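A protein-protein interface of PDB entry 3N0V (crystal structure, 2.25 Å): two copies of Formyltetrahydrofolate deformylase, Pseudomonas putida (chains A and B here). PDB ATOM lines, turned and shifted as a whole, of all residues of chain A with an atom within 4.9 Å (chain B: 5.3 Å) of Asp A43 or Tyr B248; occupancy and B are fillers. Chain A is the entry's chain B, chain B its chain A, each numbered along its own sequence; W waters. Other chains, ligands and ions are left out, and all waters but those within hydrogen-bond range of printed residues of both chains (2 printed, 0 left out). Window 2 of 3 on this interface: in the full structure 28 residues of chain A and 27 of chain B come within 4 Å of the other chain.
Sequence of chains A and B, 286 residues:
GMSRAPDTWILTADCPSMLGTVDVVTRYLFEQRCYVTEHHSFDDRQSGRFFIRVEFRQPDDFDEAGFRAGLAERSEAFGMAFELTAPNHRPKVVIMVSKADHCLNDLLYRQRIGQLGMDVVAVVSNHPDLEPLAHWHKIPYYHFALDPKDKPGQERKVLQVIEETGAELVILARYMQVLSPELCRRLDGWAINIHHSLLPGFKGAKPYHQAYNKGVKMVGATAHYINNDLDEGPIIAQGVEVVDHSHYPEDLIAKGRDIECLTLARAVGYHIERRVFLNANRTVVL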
ATOM      1  N   SER A  17     -15.479 -13.013  -1.593  1.00  0.00           N
ATOM      2  CA  SER A  17     -16.208 -12.861  -0.340  1.00  0.00           C
ATOM      3  C   SER A  17     -16.492 -14.201   0.336  1.00  0.00           C
ATOM      4  O   SER A  17     -17.103 -15.082  -0.269  1.00  0.00           O
ATOM      5  CB  SER A  17     -17.532 -12.159  -0.605  1.00  0.00           C
ATOM      6  OG  SER A  17     -17.333 -10.937  -1.289  1.00  0.00           O
ATOM      7  N   SER A  41     -12.539  -1.566   5.559  1.00  0.00           N
ATOM      8  CA  SER A  41     -12.900  -2.682   4.696  1.00  0.00           C
ATOM      9  C   SER A  41     -14.294  -2.525   4.120  1.00  0.00           C
ATOM     10  O   SER A  41     -15.114  -1.776   4.650  1.00  0.00           O
ATOM     11  CB  SER A  41     -12.828  -3.999   5.463  1.00  0.00           C
ATOM     12  OG  SER A  41     -14.084  -4.297   6.032  1.00  0.00           O
ATOM     13  N   PHE A  42     -14.543  -3.263   3.039  1.00  0.00           N
ATOM     14  CA  PHE A  42     -15.812  -3.225   2.317  1.00  0.00           C
ATOM     15  C   PHE A  42     -16.055  -4.578   1.624  1.00  0.00           C
ATOM     16  O   PHE A  42     -15.165  -5.121   0.952  1.00  0.00           O
ATOM     17  CB  PHE A  42     -15.796  -2.065   1.309  1.00  0.00           C
ATOM     18  CG  PHE A  42     -17.016  -1.992   0.436  1.00  0.00           C
ATOM     19  CD1 PHE A  42     -18.240  -1.597   0.962  1.00  0.00           C
ATOM     20  CD2 PHE A  42     -16.944  -2.316  -0.912  1.00  0.00           C
ATOM     21  CE1 PHE A  42     -19.373  -1.531   0.159  1.00  0.00           C
ATOM     22  CE2 PHE A  42     -18.073  -2.247  -1.729  1.00  0.00           C
ATOM     23  CZ  PHE A  42     -19.285  -1.853  -1.193  1.00  0.00           C
ATOM     24  N   ASP A  43     -17.251  -5.130   1.823  1.00  0.00           N
ATOM     25  CA  ASP A  43     -17.666  -6.383   1.180  1.00  0.00           C
ATOM     26  C   ASP A  43     -18.757  -6.038   0.176  1.00  0.00           C
ATOM     27  O   ASP A  43     -19.866  -5.692   0.552  1.00  0.00           O
ATOM     28  CB  ASP A  43     -18.180  -7.385   2.220  1.00  0.00           C
ATOM     29  CG  ASP A  43     -18.346  -8.775   1.659  1.00  0.00           C
ATOM     30  OD1 ASP A  43     -17.331  -9.476   1.502  1.00  0.00           O
ATOM     31  OD2 ASP A  43     -19.491  -9.174   1.375  1.00  0.00           O
ATOM     32  N   ASP A  44     -18.414  -6.104  -1.104  1.00  0.00           N
ATOM     33  CA  ASP A  44     -19.329  -5.765  -2.185  1.00  0.00           C
ATOM     34  C   ASP A  44     -20.247  -6.964  -2.402  1.00  0.00           C
ATOM     35  O   ASP A  44     -19.788  -8.013  -2.851  1.00  0.00           O
ATOM     36  CB  ASP A  44     -18.518  -5.453  -3.449  1.00  0.00           C
ATOM     37  CG  ASP A  44     -19.353  -4.831  -4.555  1.00  0.00           C
ATOM     38  OD1 ASP A  44     -20.549  -5.183  -4.679  1.00  0.00           O
ATOM     39  OD2 ASP A  44     -18.797  -3.996  -5.314  1.00  0.00           O
ATOM     40  N   ARG A  45     -21.532  -6.814  -2.074  1.00  0.00           N
ATOM     41  CA  ARG A  45     -22.481  -7.921  -2.228  1.00  0.00           C
ATOM     42  C   ARG A  45     -22.886  -8.170  -3.693  1.00  0.00           C
ATOM     43  O   ARG A  45     -23.409  -9.238  -4.017  1.00  0.00           O
ATOM     44  CB  ARG A  45     -23.714  -7.743  -1.327  1.00  0.00           C
ATOM     45  CG  ARG A  45     -24.717  -6.690  -1.766  1.00  0.00           C
ATOM     46  CD  ARG A  45     -26.130  -7.011  -1.267  1.00  0.00           C
ATOM     47  NE  ARG A  45     -27.115  -6.066  -1.801  1.00  0.00           N
ATOM     48  CZ  ARG A  45     -27.412  -4.874  -1.275  1.00  0.00           C
ATOM     49  NH1 ARG A  45     -26.815  -4.437  -0.168  1.00  0.00           N
ATOM     50  NH2 ARG A  45     -28.322  -4.106  -1.863  1.00  0.00           N
ATOM     51  N   GLN A  46     -22.626  -7.203  -4.573  1.00  0.00           N
ATOM     52  CA  GLN A  46     -22.912  -7.372  -6.004  1.00  0.00           C
ATOM     53  C   GLN A  46     -21.790  -8.088  -6.773  1.00  0.00           C
ATOM     54  O   GLN A  46     -22.073  -8.943  -7.602  1.00  0.00           O
ATOM     55  CB  GLN A  46     -23.200  -6.022  -6.670  1.00  0.00           C
ATOM     56  CG  GLN A  46     -24.505  -5.348  -6.204  1.00  0.00           C
ATOM     57  CD  GLN A  46     -25.623  -5.362  -7.243  1.00  0.00           C
ATOM     58  OE1 GLN A  46     -25.387  -5.501  -8.452  1.00  0.00           O
ATOM     59  NE2 GLN A  46     -26.853  -5.190  -6.769  1.00  0.00           N
ATOM     60  N   ARG A  49     -16.743  -9.587  -3.969  1.00  0.00           N
ATOM     61  CA  ARG A  49     -15.349  -9.312  -3.619  1.00  0.00           C
ATOM     62  C   ARG A  49     -15.271  -8.574  -2.286  1.00  0.00           C
ATOM     63  O   ARG A  49     -16.134  -7.749  -1.962  1.00  0.00           O
ATOM     64  CB  ARG A  49     -14.690  -8.442  -4.692  1.00  0.00           C
ATOM     65  CG  ARG A  49     -14.877  -8.923  -6.122  1.00  0.00           C
ATOM     66  CD  ARG A  49     -14.195 -10.254  -6.364  1.00  0.00           C
ATOM     67  NE  ARG A  49     -12.801 -10.207  -5.946  1.00  0.00           N
ATOM     68  CZ  ARG A  49     -12.022 -11.271  -5.797  1.00  0.00           C
ATOM     69  NH1 ARG A  49     -12.478 -12.489  -6.059  1.00  0.00           N
ATOM     70  NH2 ARG A  49     -10.769 -11.110  -5.392  1.00  0.00           N
ATOM     71  N   PHE A  50     -14.222  -8.864  -1.528  1.00  0.00           N
ATOM     72  CA  PHE A  50     -13.980  -8.251  -0.229  1.00  0.00           C
ATOM     73  C   PHE A  50     -12.689  -7.483  -0.359  1.00  0.00           C
ATOM     74  O   PHE A  50     -11.754  -7.947  -1.023  1.00  0.00           O
ATOM     75  CB  PHE A  50     -13.836  -9.326   0.855  1.00  0.00           C
ATOM     76  CG  PHE A  50     -13.177  -8.835   2.126  1.00  0.00           C
ATOM     77  CD1 PHE A  50     -13.918  -8.186   3.109  1.00  0.00           C
ATOM     78  CD2 PHE A  50     -11.815  -9.026   2.340  1.00  0.00           C
ATOM     79  CE1 PHE A  50     -13.305  -7.723   4.280  1.00  0.00           C
ATOM     80  CE2 PHE A  50     -11.199  -8.568   3.512  1.00  0.00           C
ATOM     81  CZ  PHE A  50     -11.947  -7.917   4.477  1.00  0.00           C
ATOM     82  N   TYR B 212     -24.444   2.418 -11.357  1.00  0.00           N
ATOM     83  CA  TYR B 212     -23.780   1.482 -10.434  1.00  0.00           C
ATOM     84  C   TYR B 212     -22.744   0.598 -11.137  1.00  0.00           C
ATOM     85  O   TYR B 212     -21.591   0.550 -10.728  1.00  0.00           O
ATOM     86  CB  TYR B 212     -24.792   0.582  -9.721  1.00  0.00           C
ATOM     87  CG  TYR B 212     -24.142  -0.366  -8.727  1.00  0.00           C
ATOM     88  CD1 TYR B 212     -23.541   0.123  -7.569  1.00  0.00           C
ATOM     89  CD2 TYR B 212     -24.099  -1.742  -8.957  1.00  0.00           C
ATOM     90  CE1 TYR B 212     -22.934  -0.725  -6.657  1.00  0.00           C
ATOM     91  CE2 TYR B 212     -23.490  -2.606  -8.045  1.00  0.00           C
ATOM     92  CZ  TYR B 212     -22.904  -2.087  -6.898  1.00  0.00           C
ATOM     93  OH  TYR B 212     -22.294  -2.918  -5.975  1.00  0.00           O
ATOM     94  N   HIS B 245     -18.485   3.628  -4.026  1.00  0.00           N
ATOM     95  CA  HIS B 245     -18.650   2.169  -4.119  1.00  0.00           C
ATOM     96  C   HIS B 245     -19.684   1.540  -3.158  1.00  0.00           C
ATOM     97  O   HIS B 245     -20.287   0.512  -3.487  1.00  0.00           O
ATOM     98  CB  HIS B 245     -17.291   1.494  -3.902  1.00  0.00           C
ATOM     99  CG  HIS B 245     -16.685   1.788  -2.567  1.00  0.00           C
ATOM    100  ND1 HIS B 245     -15.826   2.846  -2.353  1.00  0.00           N
ATOM    101  CD2 HIS B 245     -16.832   1.178  -1.370  1.00  0.00           C
ATOM    102  CE1 HIS B 245     -15.462   2.865  -1.085  1.00  0.00           C
ATOM    103  NE2 HIS B 245     -16.059   1.864  -0.466  1.00  0.00           N
ATOM    104  N   SER B 246     -19.877   2.133  -1.977  1.00  0.00           N
ATOM    105  CA  SER B 246     -20.805   1.567  -0.985  1.00  0.00           C
ATOM    106  C   SER B 246     -22.257   1.928  -1.266  1.00  0.00           C
ATOM    107  O   SER B 246     -23.164   1.396  -0.623  1.00  0.00           O
ATOM    108  CB  SER B 246     -20.423   1.985   0.446  1.00  0.00           C
ATOM    109  OG  SER B 246     -20.718   3.351   0.701  1.00  0.00           O
ATOM    110  N   HIS B 247     -22.474   2.832  -2.222  1.00  0.00           N
ATOM    111  CA  HIS B 247     -23.814   3.173  -2.677  1.00  0.00           C
ATOM    112  C   HIS B 247     -24.331   2.151  -3.699  1.00  0.00           C
ATOM    113  O   HIS B 247     -23.983   2.192  -4.878  1.00  0.00           O
ATOM    114  CB  HIS B 247     -23.842   4.581  -3.295  1.00  0.00           C
ATOM    115  CG  HIS B 247     -23.665   5.687  -2.301  1.00  0.00           C
ATOM    116  ND1 HIS B 247     -22.485   5.898  -1.623  1.00  0.00           N
ATOM    117  CD2 HIS B 247     -24.515   6.654  -1.883  1.00  0.00           C
ATOM    118  CE1 HIS B 247     -22.618   6.938  -0.821  1.00  0.00           C
ATOM    119  NE2 HIS B 247     -23.840   7.417  -0.962  1.00  0.00           N
ATOM    120  N   TYR B 248     -25.180   1.243  -3.235  1.00  0.00           N
ATOM    121  CA  TYR B 248     -25.859   0.297  -4.121  1.00  0.00           C
ATOM    122  C   TYR B 248     -26.955   1.040  -4.897  1.00  0.00           C
ATOM    123  O   TYR B 248     -27.215   2.214  -4.614  1.00  0.00           O
ATOM    124  CB  TYR B 248     -26.396  -0.872  -3.299  1.00  0.00           C
ATOM    125  CG  TYR B 248     -25.277  -1.676  -2.678  1.00  0.00           C
ATOM    126  CD1 TYR B 248     -24.572  -2.615  -3.431  1.00  0.00           C
ATOM    127  CD2 TYR B 248     -24.902  -1.483  -1.348  1.00  0.00           C
ATOM    128  CE1 TYR B 248     -23.534  -3.356  -2.870  1.00  0.00           C
ATOM    129  CE2 TYR B 248     -23.872  -2.218  -0.781  1.00  0.00           C
ATOM    130  CZ  TYR B 248     -23.189  -3.154  -1.548  1.00  0.00           C
ATOM    131  OH  TYR B 248     -22.162  -3.895  -0.997  1.00  0.00           O
ATOM    132  N   PRO B 249     -27.569   0.389  -5.903  1.00  0.00           N
ATOM    133  CA  PRO B 249     -28.573   1.041  -6.752  1.00  0.00           C
ATOM    134  C   PRO B 249     -29.609   1.863  -6.000  1.00  0.00           C
ATOM    135  O   PRO B 249     -29.888   3.003  -6.383  1.00  0.00           O
ATOM    136  CB  PRO B 249     -29.238  -0.139  -7.450  1.00  0.00           C
ATOM    137  CG  PRO B 249     -28.136  -1.106  -7.606  1.00  0.00           C
ATOM    138  CD  PRO B 249     -27.291  -0.981  -6.369  1.00  0.00           C
ATOM    139  N   GLU B 250     -30.153   1.304  -4.928  1.00  0.00           N
ATOM    140  CA  GLU B 250     -31.202   1.985  -4.167  1.00  0.00           C
ATOM    141  C   GLU B 250     -30.633   3.226  -3.482  1.00  0.00           C
ATOM    142  O   GLU B 250     -31.307   4.249  -3.376  1.00  0.00           O
ATOM    143  CB  GLU B 250     -31.862   1.038  -3.149  1.00  0.00           C
ATOM    144  CG  GLU B 250     -32.287  -0.315  -3.752  1.00  0.00           C
ATOM    145  CD  GLU B 250     -33.664  -0.785  -3.304  1.00  0.00           C
ATOM    146  OE1 GLU B 250     -34.643  -0.021  -3.481  1.00  0.00           O
ATOM    147  OE2 GLU B 250     -33.768  -1.930  -2.803  1.00  0.00           O
ATOM    148  N   ASP B 251     -29.385   3.123  -3.022  1.00  0.00           N
ATOM    149  CA  ASP B 251     -28.681   4.257  -2.439  1.00  0.00           C
ATOM    150  C   ASP B 251     -28.453   5.330  -3.496  1.00  0.00           C
ATOM    151  O   ASP B 251     -28.642   6.521  -3.223  1.00  0.00           O
ATOM    152  CB  ASP B 251     -27.342   3.820  -1.840  1.00  0.00           C
ATOM    153  CG  ASP B 251     -27.501   2.783  -0.734  1.00  0.00           C
ATOM    154  OD1 ASP B 251     -28.315   3.009   0.189  1.00  0.00           O
ATOM    155  OD2 ASP B 251     -26.808   1.747  -0.787  1.00  0.00           O
ATOM    156  N   LEU B 252     -28.041   4.901  -4.693  1.00  0.00           N
ATOM    157  CA  LEU B 252     -27.822   5.812  -5.809  1.00  0.00           C
ATOM    158  C   LEU B 252     -29.123   6.488  -6.203  1.00  0.00           C
ATOM    159  O   LEU B 252     -29.165   7.722  -6.287  1.00  0.00           O
ATOM    160  CB  LEU B 252     -27.198   5.102  -7.020  1.00  0.00           C
ATOM    161  CG  LEU B 252     -25.686   4.825  -7.026  1.00  0.00           C
ATOM    162  CD1 LEU B 252     -25.241   4.404  -8.424  1.00  0.00           C
ATOM    163  CD2 LEU B 252     -24.904   6.019  -6.606  1.00  0.00           C
ATOM    164  N   ILE B 253     -30.185   5.702  -6.428  1.00  0.00           N
ATOM    165  CA  ILE B 253     -31.510   6.289  -6.646  1.00  0.00           C
ATOM    166  C   ILE B 253     -31.810   7.317  -5.563  1.00  0.00           C
ATOM    167  O   ILE B 253     -32.265   8.413  -5.868  1.00  0.00           O
ATOM    168  CB  ILE B 253     -32.647   5.253  -6.672  1.00  0.00           C
ATOM    169  CG1 ILE B 253     -32.543   4.358  -7.904  1.00  0.00           C
ATOM    170  CG2 ILE B 253     -34.014   5.948  -6.695  1.00  0.00           C
ATOM    171  CD1 ILE B 253     -33.441   3.097  -7.827  1.00  0.00           C
HETATM  172  O   HOH W   1     -19.908  -1.574  -5.042  1.00  0.00           O
HETATM  173  O   HOH W   2     -21.425  -4.141   1.780  1.00  0.00           O
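The side-chain hydroxyl (OH) of Tyr B248 lies within hydrogen-bond range of the backbone NH (N) of Arg A45 (3.2 Å).
The side-chain hydroxyl (OH) of Tyr B212 sits at hydrogen-bond distance from the side-chain carboxylate (OD1) of Asp A44 (3.1 Å).
The side-chain hydroxyl (OH) of Tyr B248 is in hydrogen-bond range of the backbone carbonyl oxygen (O) of Asp A43, at 3.3 Å.
The side-chain carboxylate (OD2) of Asp B251 sits at hydrogen-bond distance from the backbone NH (N) of Tyr B248, 3.0 Å away.
O of Arg A49 is in hydrogen-bond range of N of Asp A44 (2.9 Å).
The backbone NH (N) of Gln A46 sits at hydrogen-bond distance from the side-chain carboxylate (OD1) of Asp A44.
The side-chain carboxylate (OD1) of Asp A43 is in hydrogen-bond range of the side-chain hydroxyl (OG) of Ser A17 (3.2 Å).
Among the printed residues, pairs that only touch across the chains: Gln A46 with Tyr B212 (3.3 Å), Phe A42 with His B245 (3.4 Å), Phe A42 with Tyr B248 (3.5 Å), Asp A44 with Tyr B248 (3.6 Å), Phe A42 with Ser B246 (3.6 Å) and Gln A46 with Tyr B248 (3.9 Å).
Asp A43 touches one residue of chain B.
Of the printed residues of chain B, Asp A44 touches Tyr B212 (3.1 Å) and Tyr B248 (3.6 Å).
Of the printed residues of chain B, Gln A46 touches Tyr B212 (3.3 Å) and Tyr B248 (3.9 Å).
Tyr B248 touches just these residues of chain A: Phe A42, Asp A43, Asp A44, Arg A45 and Gln A46.
The nearest printed residue of chain A that does not touch Tyr B248 is Arg A49 (7.2 Å).
Along chain B the printed residues that touch a printed residue of chain A span positions 212 to 248.
Of the 9 printed residues of chain A, 5 touch a printed residue of chain B.
Printed residues of chain A that touch a printed residue of chain B: Phe A42, Asp A43, Asp A44, Arg A45 and Gln A46.
Hydrophobic or aromatic side chains of chain A that line the printed part of chain B: Phe A42.
Among the printed residues, 9 pairs touch across the chains.
Among the printed residues, no Asp or Glu carboxylate lies within 4 Å of a Lys or Arg side-chain nitrogen of the other chain.
No position is printed for both chains.
Of the 9 pairs that touch across the chains among the printed residues, none has its exchanged pair printed and touching as well.
Water W2 lies within hydrogen-bond range of O of Asp A43 (2.5 Å) and OH of Tyr B248 (2.9 Å).
Water W1 lies within hydrogen-bond range of O of His B245, OD2 of Asp A44 and OH of Tyr B212.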
